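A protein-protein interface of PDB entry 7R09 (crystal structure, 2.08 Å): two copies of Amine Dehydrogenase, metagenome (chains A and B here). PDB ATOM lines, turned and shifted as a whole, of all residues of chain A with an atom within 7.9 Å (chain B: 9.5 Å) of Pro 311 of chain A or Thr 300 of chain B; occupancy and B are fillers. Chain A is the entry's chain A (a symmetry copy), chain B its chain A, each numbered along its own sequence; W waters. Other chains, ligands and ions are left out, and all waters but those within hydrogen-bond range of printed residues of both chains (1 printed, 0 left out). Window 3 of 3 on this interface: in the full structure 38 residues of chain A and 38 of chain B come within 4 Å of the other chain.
O of Met 158 of chain B is in hydrogen-bond range of OG1 of Thr 318 of chain A (2.8 Å).
N of Val 303 of chain B lies close to OD1 of Asn 294 of chain B. O of Met 315 of chain A sits at hydrogen-bond distance from OG1 of Thr 318 of chain A, at 3.0 Å. The backbone carbonyl oxygen of Asn 298 of chain B sits at hydrogen-bond distance from the backbone NH of His 160 of chain B, 2.5 Å away. N of Asn 298 of chain B lies within hydrogen-bond range of O of Lys 161 of chain B, at 2.8 Å. The backbone carbonyl oxygen of Val 303 of chain B lies within hydrogen-bond range of the backbone NH of Leu 295 of chain B (2.8 Å). OD1 of Asn 294 of chain B is in hydrogen-bond range of N of Gly 304 of chain B, at 3.4 Å.
Among the printed residues, pairs that only touch across the chains: Met 27 of chain A with His 160 of chain B, Met 27 of chain A with Asn 298 of chain B, Met 307 of chain A with Gly 304 of chain B, Pro 311 of chain A with Pro 299 of chain B, Pro 311 of chain A with Thr 300 of chain B, Pro 311 of chain A with Gly 302 of chain B, Pro 311 of chain A with Val 303 of chain B, Ala 314 of chain A with Pro 299 of chain B, Met 315 of chain A with Met 158 of chain B and Thr 318 of chain A with Pro 299 of chain B.
Of the printed residues of chain B, Met 307 of chain A touches Gly 304 (3.3 Å). Lys 308 of chain A touches none of the printed residues of chain B. Pro 311 of chain A touches four residues of chain B. No residue of chain B comes within 4 Å of Thr 312 of chain A. Of chain B, only Pro 299 (3.8 Å) comes within 4 Å of Ala 314 of chain A. Printed residues of chain B within 4 Å of Met 315 of chain A: Met 158. Of the printed residues of chain A, Asn 298 of chain B touches Met 27. Thr 300 of chain B touches just one residue of chain A: Pro 311 (3.7 Å). Of the printed residues of chain A, Gly 304 of chain B touches Met 307. The nearest residue of chain B that does not touch Pro 311 of chain A is Gly 301 of chain B (5.8 Å). The nearest printed residue of chain B that does not touch Thr 318 of chain A is His 160 of chain B (4.2 Å).
Of the 18 printed residues of chain B, 8 touch a printed residue of chain A. Hydrophobic or aromatic side chains of chain B that line the printed part of chain A: Met 158, His 160, Pro 299 and Val 303. Of the 16 printed residues of chain A, 6 touch a printed residue of chain B. Among the printed residues, no Asp or Glu carboxylate lies within 4 Å of a Lys or Arg side-chain nitrogen of the other chain.
No position is printed for both chains. Of the 11 pairs that touch across the chains among the printed residues, none has its exchanged pair printed and touching as well.
Water W1 bridges the backbone carbonyl oxygen (O) of Gly 304 of chain B (3.3 Å) and the backbone NH (N) of Lys 308 of chain A (3.3 Å).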
ATOM      1  N   MET A  27     -16.715 -35.902  18.255  1.00  0.00           N
ATOM      2  CA  MET A  27     -15.545 -36.565  17.632  1.00  0.00           C
ATOM      3  C   MET A  27     -14.818 -37.386  18.701  1.00  0.00           C
ATOM      4  O   MET A  27     -14.417 -38.524  18.400  1.00  0.00           O
ATOM      5  CB  MET A  27     -14.603 -35.528  17.011  1.00  0.00           C
ATOM      6  CG  MET A  27     -15.248 -34.764  15.864  1.00  0.00           C
ATOM      7  SD  MET A  27     -14.109 -33.567  15.109  1.00  0.00           S
ATOM      8  CE  MET A  27     -14.973 -33.204  13.577  1.00  0.00           C
ATOM      9  N   PHE A 143      -7.180 -23.057  15.551  1.00  0.00           N
ATOM     10  CA  PHE A 143      -7.046 -22.806  14.092  1.00  0.00           C
ATOM     11  C   PHE A 143      -5.764 -22.032  13.766  1.00  0.00           C
ATOM     12  O   PHE A 143      -5.178 -22.285  12.701  1.00  0.00           O
ATOM     13  CB  PHE A 143      -8.234 -21.998  13.568  1.00  0.00           C
ATOM     14  CG  PHE A 143      -8.337 -22.014  12.066  1.00  0.00           C
ATOM     15  CD1 PHE A 143      -8.627 -23.190  11.385  1.00  0.00           C
ATOM     16  CD2 PHE A 143      -8.149 -20.858  11.317  1.00  0.00           C
ATOM     17  CE1 PHE A 143      -8.745 -23.207  10.001  1.00  0.00           C
ATOM     18  CE2 PHE A 143      -8.244 -20.882   9.934  1.00  0.00           C
ATOM     19  CZ  PHE A 143      -8.534 -22.053   9.276  1.00  0.00           C
ATOM     20  N   TYR A 176     -19.802 -17.096  15.100  1.00  0.00           N
ATOM     21  CA  TYR A 176     -19.181 -17.444  16.411  1.00  0.00           C
ATOM     22  C   TYR A 176     -19.921 -16.727  17.548  1.00  0.00           C
ATOM     23  O   TYR A 176     -19.348 -16.649  18.667  1.00  0.00           O
ATOM     24  CB  TYR A 176     -17.680 -17.121  16.423  1.00  0.00           C
ATOM     25  CG  TYR A 176     -16.886 -17.818  15.348  1.00  0.00           C
ATOM     26  CD1 TYR A 176     -16.991 -17.409  14.033  1.00  0.00           C
ATOM     27  CD2 TYR A 176     -16.080 -18.914  15.627  1.00  0.00           C
ATOM     28  CE1 TYR A 176     -16.314 -18.059  13.019  1.00  0.00           C
ATOM     29  CE2 TYR A 176     -15.378 -19.568  14.622  1.00  0.00           C
ATOM     30  CZ  TYR A 176     -15.499 -19.135  13.310  1.00  0.00           C
ATOM     31  OH  TYR A 176     -14.866 -19.746  12.265  1.00  0.00           O
ATOM     32  N   ASP A 289     -14.301 -18.274   3.774  1.00  0.00           N
ATOM     33  CA  ASP A 289     -13.109 -18.389   4.646  1.00  0.00           C
ATOM     34  C   ASP A 289     -11.897 -18.587   3.730  1.00  0.00           C
ATOM     35  O   ASP A 289     -12.065 -19.123   2.612  1.00  0.00           O
ATOM     36  CB  ASP A 289     -13.250 -19.502   5.687  1.00  0.00           C
ATOM     37  CG  ASP A 289     -14.244 -19.217   6.800  1.00  0.00           C
ATOM     38  OD1 ASP A 289     -15.068 -18.297   6.640  1.00  0.00           O
ATOM     39  OD2 ASP A 289     -14.183 -19.921   7.823  1.00  0.00           O
ATOM     40  N   MET A 307      -5.542 -21.998   1.354  1.00  0.00           N
ATOM     41  CA  MET A 307      -6.656 -22.936   1.669  1.00  0.00           C
ATOM     42  C   MET A 307      -7.957 -22.182   1.433  1.00  0.00           C
ATOM     43  O   MET A 307      -8.185 -21.175   2.125  1.00  0.00           O
ATOM     44  CB  MET A 307      -6.634 -23.425   3.120  1.00  0.00           C
ATOM     45  CG  MET A 307      -5.398 -24.219   3.493  1.00  0.00           C
ATOM     46  SD  MET A 307      -5.480 -24.995   5.136  1.00  0.00           S
ATOM     47  CE  MET A 307      -7.014 -24.318   5.760  1.00  0.00           C
ATOM     48  N   LYS A 308      -8.736 -22.619   0.448  1.00  0.00           N
ATOM     49  CA  LYS A 308     -10.003 -21.959   0.050  1.00  0.00           C
ATOM     50  C   LYS A 308     -11.113 -22.596   0.880  1.00  0.00           C
ATOM     51  O   LYS A 308     -11.070 -23.820   1.062  1.00  0.00           O
ATOM     52  CB  LYS A 308     -10.225 -22.096  -1.462  1.00  0.00           C
ATOM     53  N   ASN A 309     -12.001 -21.784   1.448  1.00  0.00           N
ATOM     54  CA  ASN A 309     -13.221 -22.257   2.143  1.00  0.00           C
ATOM     55  C   ASN A 309     -12.914 -23.419   3.094  1.00  0.00           C
ATOM     56  O   ASN A 309     -13.583 -24.452   3.078  1.00  0.00           O
ATOM     57  CB  ASN A 309     -14.275 -22.668   1.115  1.00  0.00           C
ATOM     58  CG  ASN A 309     -15.614 -22.907   1.766  1.00  0.00           C
ATOM     59  OD1 ASN A 309     -16.163 -22.004   2.388  1.00  0.00           O
ATOM     60  ND2 ASN A 309     -16.113 -24.130   1.674  1.00  0.00           N
ATOM     61  N   PRO A 310     -11.942 -23.288   4.017  1.00  0.00           N
ATOM     62  CA  PRO A 310     -11.755 -24.313   5.042  1.00  0.00           C
ATOM     63  C   PRO A 310     -12.855 -24.305   6.107  1.00  0.00           C
ATOM     64  O   PRO A 310     -13.266 -23.242   6.573  1.00  0.00           O
ATOM     65  CB  PRO A 310     -10.400 -23.937   5.645  1.00  0.00           C
ATOM     66  CG  PRO A 310     -10.354 -22.425   5.509  1.00  0.00           C
ATOM     67  CD  PRO A 310     -11.033 -22.142   4.183  1.00  0.00           C
ATOM     68  N   PRO A 311     -13.361 -25.489   6.524  1.00  0.00           N
ATOM     69  CA  PRO A 311     -14.329 -25.591   7.616  1.00  0.00           C
ATOM     70  C   PRO A 311     -13.694 -25.236   8.962  1.00  0.00           C
ATOM     71  O   PRO A 311     -13.385 -26.136   9.763  1.00  0.00           O
ATOM     72  CB  PRO A 311     -14.741 -27.068   7.564  1.00  0.00           C
ATOM     73  CG  PRO A 311     -13.502 -27.751   7.019  1.00  0.00           C
ATOM     74  CD  PRO A 311     -13.043 -26.801   5.936  1.00  0.00           C
ATOM     75  N   THR A 312     -13.501 -23.928   9.173  1.00  0.00           N
ATOM     76  CA  THR A 312     -12.668 -23.350  10.253  1.00  0.00           C
ATOM     77  C   THR A 312     -13.122 -23.847  11.623  1.00  0.00           C
ATOM     78  O   THR A 312     -12.285 -24.202  12.449  1.00  0.00           O
ATOM     79  CB  THR A 312     -12.674 -21.816  10.175  1.00  0.00           C
ATOM     80  OG1 THR A 312     -12.246 -21.373   8.881  1.00  0.00           O
ATOM     81  CG2 THR A 312     -11.822 -21.211  11.262  1.00  0.00           C
ATOM     82  N   PRO A 313     -14.441 -23.807  11.962  1.00  0.00           N
ATOM     83  CA  PRO A 313     -14.919 -24.313  13.255  1.00  0.00           C
ATOM     84  C   PRO A 313     -14.495 -25.748  13.601  1.00  0.00           C
ATOM     85  O   PRO A 313     -14.060 -25.981  14.715  1.00  0.00           O
ATOM     86  CB  PRO A 313     -16.445 -24.252  13.117  1.00  0.00           C
ATOM     87  CG  PRO A 313     -16.671 -23.111  12.130  1.00  0.00           C
ATOM     88  CD  PRO A 313     -15.527 -23.230  11.151  1.00  0.00           C
ATOM     89  N   ALA A 314     -14.635 -26.677  12.655  1.00  0.00           N
ATOM     90  CA  ALA A 314     -14.326 -28.112  12.862  1.00  0.00           C
ATOM     91  C   ALA A 314     -12.806 -28.314  12.900  1.00  0.00           C
ATOM     92  O   ALA A 314     -12.304 -29.069  13.773  1.00  0.00           O
ATOM     93  CB  ALA A 314     -14.993 -28.929  11.788  1.00  0.00           C
ATOM     94  N   MET A 315     -12.064 -27.591  12.056  1.00  0.00           N
ATOM     95  CA  MET A 315     -10.578 -27.666  12.046  1.00  0.00           C
ATOM     96  C   MET A 315      -9.997 -27.194  13.392  1.00  0.00           C
ATOM     97  O   MET A 315      -8.987 -27.805  13.873  1.00  0.00           O
ATOM     98  CB  MET A 315     -10.035 -26.879  10.850  1.00  0.00           C
ATOM     99  CG  MET A 315     -10.433 -27.542   9.542  1.00  0.00           C
ATOM    100  SD  MET A 315     -10.043 -26.605   8.057  1.00  0.00           S
ATOM    101  CE  MET A 315      -8.262 -26.784   8.058  1.00  0.00           C
ATOM    102  N   THR A 316     -10.628 -26.202  14.032  1.00  0.00           N
ATOM    103  CA  THR A 316     -10.214 -25.724  15.372  1.00  0.00           C
ATOM    104  C   THR A 316     -10.232 -26.904  16.347  1.00  0.00           C
ATOM    105  O   THR A 316      -9.315 -26.992  17.227  1.00  0.00           O
ATOM    106  CB  THR A 316     -11.084 -24.561  15.871  1.00  0.00           C
ATOM    107  OG1 THR A 316     -10.920 -23.449  14.994  1.00  0.00           O
ATOM    108  CG2 THR A 316     -10.730 -24.123  17.272  1.00  0.00           C
ATOM    109  N   ASN A 317     -11.252 -27.749  16.244  1.00  0.00           N
ATOM    110  CA  ASN A 317     -11.437 -28.916  17.147  1.00  0.00           C
ATOM    111  C   ASN A 317     -10.434 -30.015  16.765  1.00  0.00           C
ATOM    112  O   ASN A 317      -9.785 -30.599  17.679  1.00  0.00           O
ATOM    113  CB  ASN A 317     -12.896 -29.389  17.123  1.00  0.00           C
ATOM    114  CG  ASN A 317     -13.858 -28.369  17.697  1.00  0.00           C
ATOM    115  OD1 ASN A 317     -13.495 -27.611  18.589  1.00  0.00           O
ATOM    116  ND2 ASN A 317     -15.087 -28.346  17.205  1.00  0.00           N
ATOM    117  N   THR A 318     -10.297 -30.318  15.471  1.00  0.00           N
ATOM    118  CA  THR A 318      -9.370 -31.394  15.013  1.00  0.00           C
ATOM    119  C   THR A 318      -7.941 -31.008  15.402  1.00  0.00           C
ATOM    120  O   THR A 318      -7.205 -31.894  15.907  1.00  0.00           O
ATOM    121  CB  THR A 318      -9.554 -31.718  13.530  1.00  0.00           C
ATOM    122  OG1 THR A 318      -9.383 -30.521  12.775  1.00  0.00           O
ATOM    123  CG2 THR A 318     -10.911 -32.313  13.232  1.00  0.00           C
ATOM    124  N   MET B 155      -1.457 -31.237   6.758  1.00  0.00           N
ATOM    125  CA  MET B 155      -2.864 -30.811   6.590  1.00  0.00           C
ATOM    126  C   MET B 155      -3.811 -31.961   6.967  1.00  0.00           C
ATOM    127  O   MET B 155      -4.884 -31.670   7.549  1.00  0.00           O
ATOM    128  CB  MET B 155      -3.147 -30.390   5.148  1.00  0.00           C
ATOM    129  CG  MET B 155      -4.558 -29.883   4.966  1.00  0.00           C
ATOM    130  SD  MET B 155      -4.926 -29.325   3.283  1.00  0.00           S
ATOM    131  CE  MET B 155      -4.731 -30.844   2.360  1.00  0.00           C
ATOM    132  N   MET B 158      -5.457 -32.697  10.437  1.00  0.00           N
ATOM    133  CA  MET B 158      -6.654 -31.924  10.842  1.00  0.00           C
ATOM    134  C   MET B 158      -7.924 -32.675  10.428  1.00  0.00           C
ATOM    135  O   MET B 158      -8.982 -32.070  10.514  1.00  0.00           O
ATOM    136  CB  MET B 158      -6.638 -30.508  10.237  1.00  0.00           C
ATOM    137  CG  MET B 158      -5.423 -29.655  10.711  1.00  0.00           C
ATOM    138  SD  MET B 158      -5.486 -27.898  10.228  1.00  0.00           S
ATOM    139  CE  MET B 158      -5.037 -28.017   8.502  1.00  0.00           C
ATOM    140  N   MET B 159      -7.831 -33.951  10.043  1.00  0.00           N
ATOM    141  CA  MET B 159      -9.006 -34.760   9.606  1.00  0.00           C
ATOM    142  C   MET B 159      -9.387 -35.692  10.758  1.00  0.00           C
ATOM    143  O   MET B 159      -8.464 -36.239  11.401  1.00  0.00           O
ATOM    144  CB  MET B 159      -8.729 -35.611   8.358  1.00  0.00           C
ATOM    145  CG  MET B 159      -8.505 -34.821   7.087  1.00  0.00           C
ATOM    146  SD  MET B 159      -9.779 -33.596   6.704  1.00  0.00           S
ATOM    147  CE  MET B 159     -11.030 -34.613   5.908  1.00  0.00           C
ATOM    148  N   HIS B 160     -10.689 -35.859  11.004  1.00  0.00           N
ATOM    149  CA  HIS B 160     -11.252 -36.873  11.943  1.00  0.00           C
ATOM    150  C   HIS B 160     -11.448 -38.186  11.177  1.00  0.00           C
ATOM    151  O   HIS B 160     -10.993 -39.227  11.666  1.00  0.00           O
ATOM    152  CB  HIS B 160     -12.526 -36.314  12.583  1.00  0.00           C
ATOM    153  CG  HIS B 160     -13.310 -37.279  13.397  1.00  0.00           C
ATOM    154  ND1 HIS B 160     -12.849 -37.778  14.592  1.00  0.00           N
ATOM    155  CD2 HIS B 160     -14.544 -37.796  13.210  1.00  0.00           C
ATOM    156  CE1 HIS B 160     -13.767 -38.565  15.109  1.00  0.00           C
ATOM    157  NE2 HIS B 160     -14.803 -38.603  14.274  1.00  0.00           N
ATOM    158  N   LYS B 161     -12.062 -38.119   9.993  1.00  0.00           N
ATOM    159  CA  LYS B 161     -12.171 -39.270   9.063  1.00  0.00           C
ATOM    160  C   LYS B 161     -11.792 -38.804   7.658  1.00  0.00           C
ATOM    161  O   LYS B 161     -12.356 -37.808   7.205  1.00  0.00           O
ATOM    162  CB  LYS B 161     -13.594 -39.849   9.053  1.00  0.00           C
ATOM    163  N   ILE B 162     -10.948 -39.558   6.956  1.00  0.00           N
ATOM    164  CA  ILE B 162     -10.720 -39.319   5.503  1.00  0.00           C
ATOM    165  C   ILE B 162     -11.363 -40.465   4.708  1.00  0.00           C
ATOM    166  O   ILE B 162     -10.980 -41.659   4.928  1.00  0.00           O
ATOM    167  CB  ILE B 162      -9.225 -39.103   5.190  1.00  0.00           C
ATOM    168  CG1 ILE B 162      -8.923 -39.281   3.707  1.00  0.00           C
ATOM    169  CG2 ILE B 162      -8.339 -39.975   6.036  1.00  0.00           C
ATOM    170  CD1 ILE B 162      -9.391 -38.118   2.908  1.00  0.00           C
ATOM    171  N   ASP B 163     -12.293 -40.087   3.820  1.00  0.00           N
ATOM    172  CA  ASP B 163     -12.976 -40.945   2.818  1.00  0.00           C
ATOM    173  C   ASP B 163     -12.189 -40.971   1.499  1.00  0.00           C
ATOM    174  O   ASP B 163     -12.171 -42.038   0.833  1.00  0.00           O
ATOM    175  CB  ASP B 163     -14.393 -40.436   2.571  1.00  0.00           C
ATOM    176  CG  ASP B 163     -15.264 -40.464   3.820  1.00  0.00           C
ATOM    177  OD1 ASP B 163     -15.031 -41.335   4.666  1.00  0.00           O
ATOM    178  OD2 ASP B 163     -16.157 -39.612   3.937  1.00  0.00           O
ATOM    179  N   ASN B 294      -6.661 -32.073  -1.662  1.00  0.00           N
ATOM    180  CA  ASN B 294      -8.005 -31.911  -1.053  1.00  0.00           C
ATOM    181  C   ASN B 294      -8.411 -33.222  -0.374  1.00  0.00           C
ATOM    182  O   ASN B 294      -8.163 -34.312  -0.941  1.00  0.00           O
ATOM    183  CB  ASN B 294      -9.026 -31.449  -2.086  1.00  0.00           C
ATOM    184  CG  ASN B 294     -10.327 -31.031  -1.429  1.00  0.00           C
ATOM    185  OD1 ASN B 294     -10.333 -30.219  -0.509  1.00  0.00           O
ATOM    186  ND2 ASN B 294     -11.434 -31.609  -1.861  1.00  0.00           N
ATOM    187  N   LEU B 295      -8.924 -33.128   0.849  1.00  0.00           N
ATOM    188  CA  LEU B 295      -9.326 -34.287   1.678  1.00  0.00           C
ATOM    189  C   LEU B 295     -10.831 -34.204   1.931  1.00  0.00           C
ATOM    190  O   LEU B 295     -11.309 -33.126   2.391  1.00  0.00           O
ATOM    191  CB  LEU B 295      -8.555 -34.284   2.998  1.00  0.00           C
ATOM    192  CG  LEU B 295      -7.049 -34.071   2.886  1.00  0.00           C
ATOM    193  CD1 LEU B 295      -6.455 -33.822   4.262  1.00  0.00           C
ATOM    194  CD2 LEU B 295      -6.373 -35.249   2.217  1.00  0.00           C
ATOM    195  N   GLU B 296     -11.541 -35.288   1.606  1.00  0.00           N
ATOM    196  CA  GLU B 296     -13.018 -35.408   1.730  1.00  0.00           C
ATOM    197  C   GLU B 296     -13.324 -36.386   2.858  1.00  0.00           C
ATOM    198  O   GLU B 296     -12.792 -37.502   2.809  1.00  0.00           O
ATOM    199  CB  GLU B 296     -13.665 -35.950   0.462  1.00  0.00           C
ATOM    200  CG  GLU B 296     -13.319 -35.203  -0.800  1.00  0.00           C
ATOM    201  CD  GLU B 296     -13.915 -35.870  -2.030  1.00  0.00           C
ATOM    202  OE1 GLU B 296     -14.850 -36.713  -1.879  1.00  0.00           O
ATOM    203  OE2 GLU B 296     -13.439 -35.565  -3.132  1.00  0.00           O
ATOM    204  N   GLY B 297     -14.189 -35.988   3.790  1.00  0.00           N
ATOM    205  CA  GLY B 297     -14.469 -36.743   5.023  1.00  0.00           C
ATOM    206  C   GLY B 297     -14.955 -35.816   6.113  1.00  0.00           C
ATOM    207  O   GLY B 297     -15.866 -35.023   5.861  1.00  0.00           O
ATOM    208  N   ASN B 298     -14.347 -35.900   7.288  1.00  0.00           N
ATOM    209  CA  ASN B 298     -14.732 -35.075   8.453  1.00  0.00           C
ATOM    210  C   ASN B 298     -13.451 -34.507   9.043  1.00  0.00           C
ATOM    211  O   ASN B 298     -12.601 -35.275   9.510  1.00  0.00           O
ATOM    212  CB  ASN B 298     -15.576 -35.905   9.422  1.00  0.00           C
ATOM    213  CG  ASN B 298     -16.131 -35.107  10.583  1.00  0.00           C
ATOM    214  OD1 ASN B 298     -15.864 -33.916  10.717  1.00  0.00           O
ATOM    215  ND2 ASN B 298     -16.871 -35.774  11.458  1.00  0.00           N
ATOM    216  N   PRO B 299     -13.253 -33.162   9.059  1.00  0.00           N
ATOM    217  CA  PRO B 299     -14.238 -32.176   8.594  1.00  0.00           C
ATOM    218  C   PRO B 299     -14.719 -32.270   7.143  1.00  0.00           C
ATOM    219  O   PRO B 299     -13.996 -32.723   6.292  1.00  0.00           O
ATOM    220  CB  PRO B 299     -13.510 -30.834   8.764  1.00  0.00           C
ATOM    221  CG  PRO B 299     -12.573 -31.095   9.906  1.00  0.00           C
ATOM    222  CD  PRO B 299     -12.085 -32.510   9.672  1.00  0.00           C
ATOM    223  N   THR B 300     -15.941 -31.797   6.912  1.00  0.00           N
ATOM    224  CA  THR B 300     -16.704 -31.987   5.652  1.00  0.00           C
ATOM    225  C   THR B 300     -16.497 -30.778   4.746  1.00  0.00           C
ATOM    226  O   THR B 300     -16.035 -29.744   5.273  1.00  0.00           O
ATOM    227  CB  THR B 300     -18.200 -32.143   5.935  1.00  0.00           C
ATOM    228  OG1 THR B 300     -18.681 -30.886   6.414  1.00  0.00           O
ATOM    229  CG2 THR B 300     -18.499 -33.217   6.955  1.00  0.00           C
ATOM    230  N   GLY B 301     -16.853 -30.916   3.461  1.00  0.00           N
ATOM    231  CA  GLY B 301     -16.824 -29.832   2.460  1.00  0.00           C
ATOM    232  C   GLY B 301     -15.525 -29.796   1.669  1.00  0.00           C
ATOM    233  O   GLY B 301     -15.492 -29.087   0.639  1.00  0.00           O
ATOM    234  N   GLY B 302     -14.508 -30.558   2.093  1.00  0.00           N
ATOM    235  CA  GLY B 302     -13.158 -30.522   1.490  1.00  0.00           C
ATOM    236  C   GLY B 302     -12.179 -29.686   2.311  1.00  0.00           C
ATOM    237  O   GLY B 302     -12.409 -28.496   2.483  1.00  0.00           O
ATOM    238  N   VAL B 303     -11.146 -30.317   2.851  1.00  0.00           N
ATOM    239  CA  VAL B 303      -9.982 -29.655   3.502  1.00  0.00           C
ATOM    240  C   VAL B 303      -8.838 -29.665   2.485  1.00  0.00           C
ATOM    241  O   VAL B 303      -8.284 -30.737   2.245  1.00  0.00           O
ATOM    242  CB  VAL B 303      -9.642 -30.397   4.797  1.00  0.00           C
ATOM    243  CG1 VAL B 303      -8.353 -29.910   5.443  1.00  0.00           C
ATOM    244  CG2 VAL B 303     -10.805 -30.300   5.765  1.00  0.00           C
ATOM    245  N   GLY B 304      -8.586 -28.529   1.830  1.00  0.00           N
ATOM    246  CA  GLY B 304      -7.700 -28.433   0.652  1.00  0.00           C
ATOM    247  C   GLY B 304      -6.628 -27.373   0.821  1.00  0.00           C
ATOM    248  O   GLY B 304      -6.886 -26.361   1.504  1.00  0.00           O
HETATM  249  O   HOH W   1      -7.660 -25.121  -1.410  1.00  0.00           O
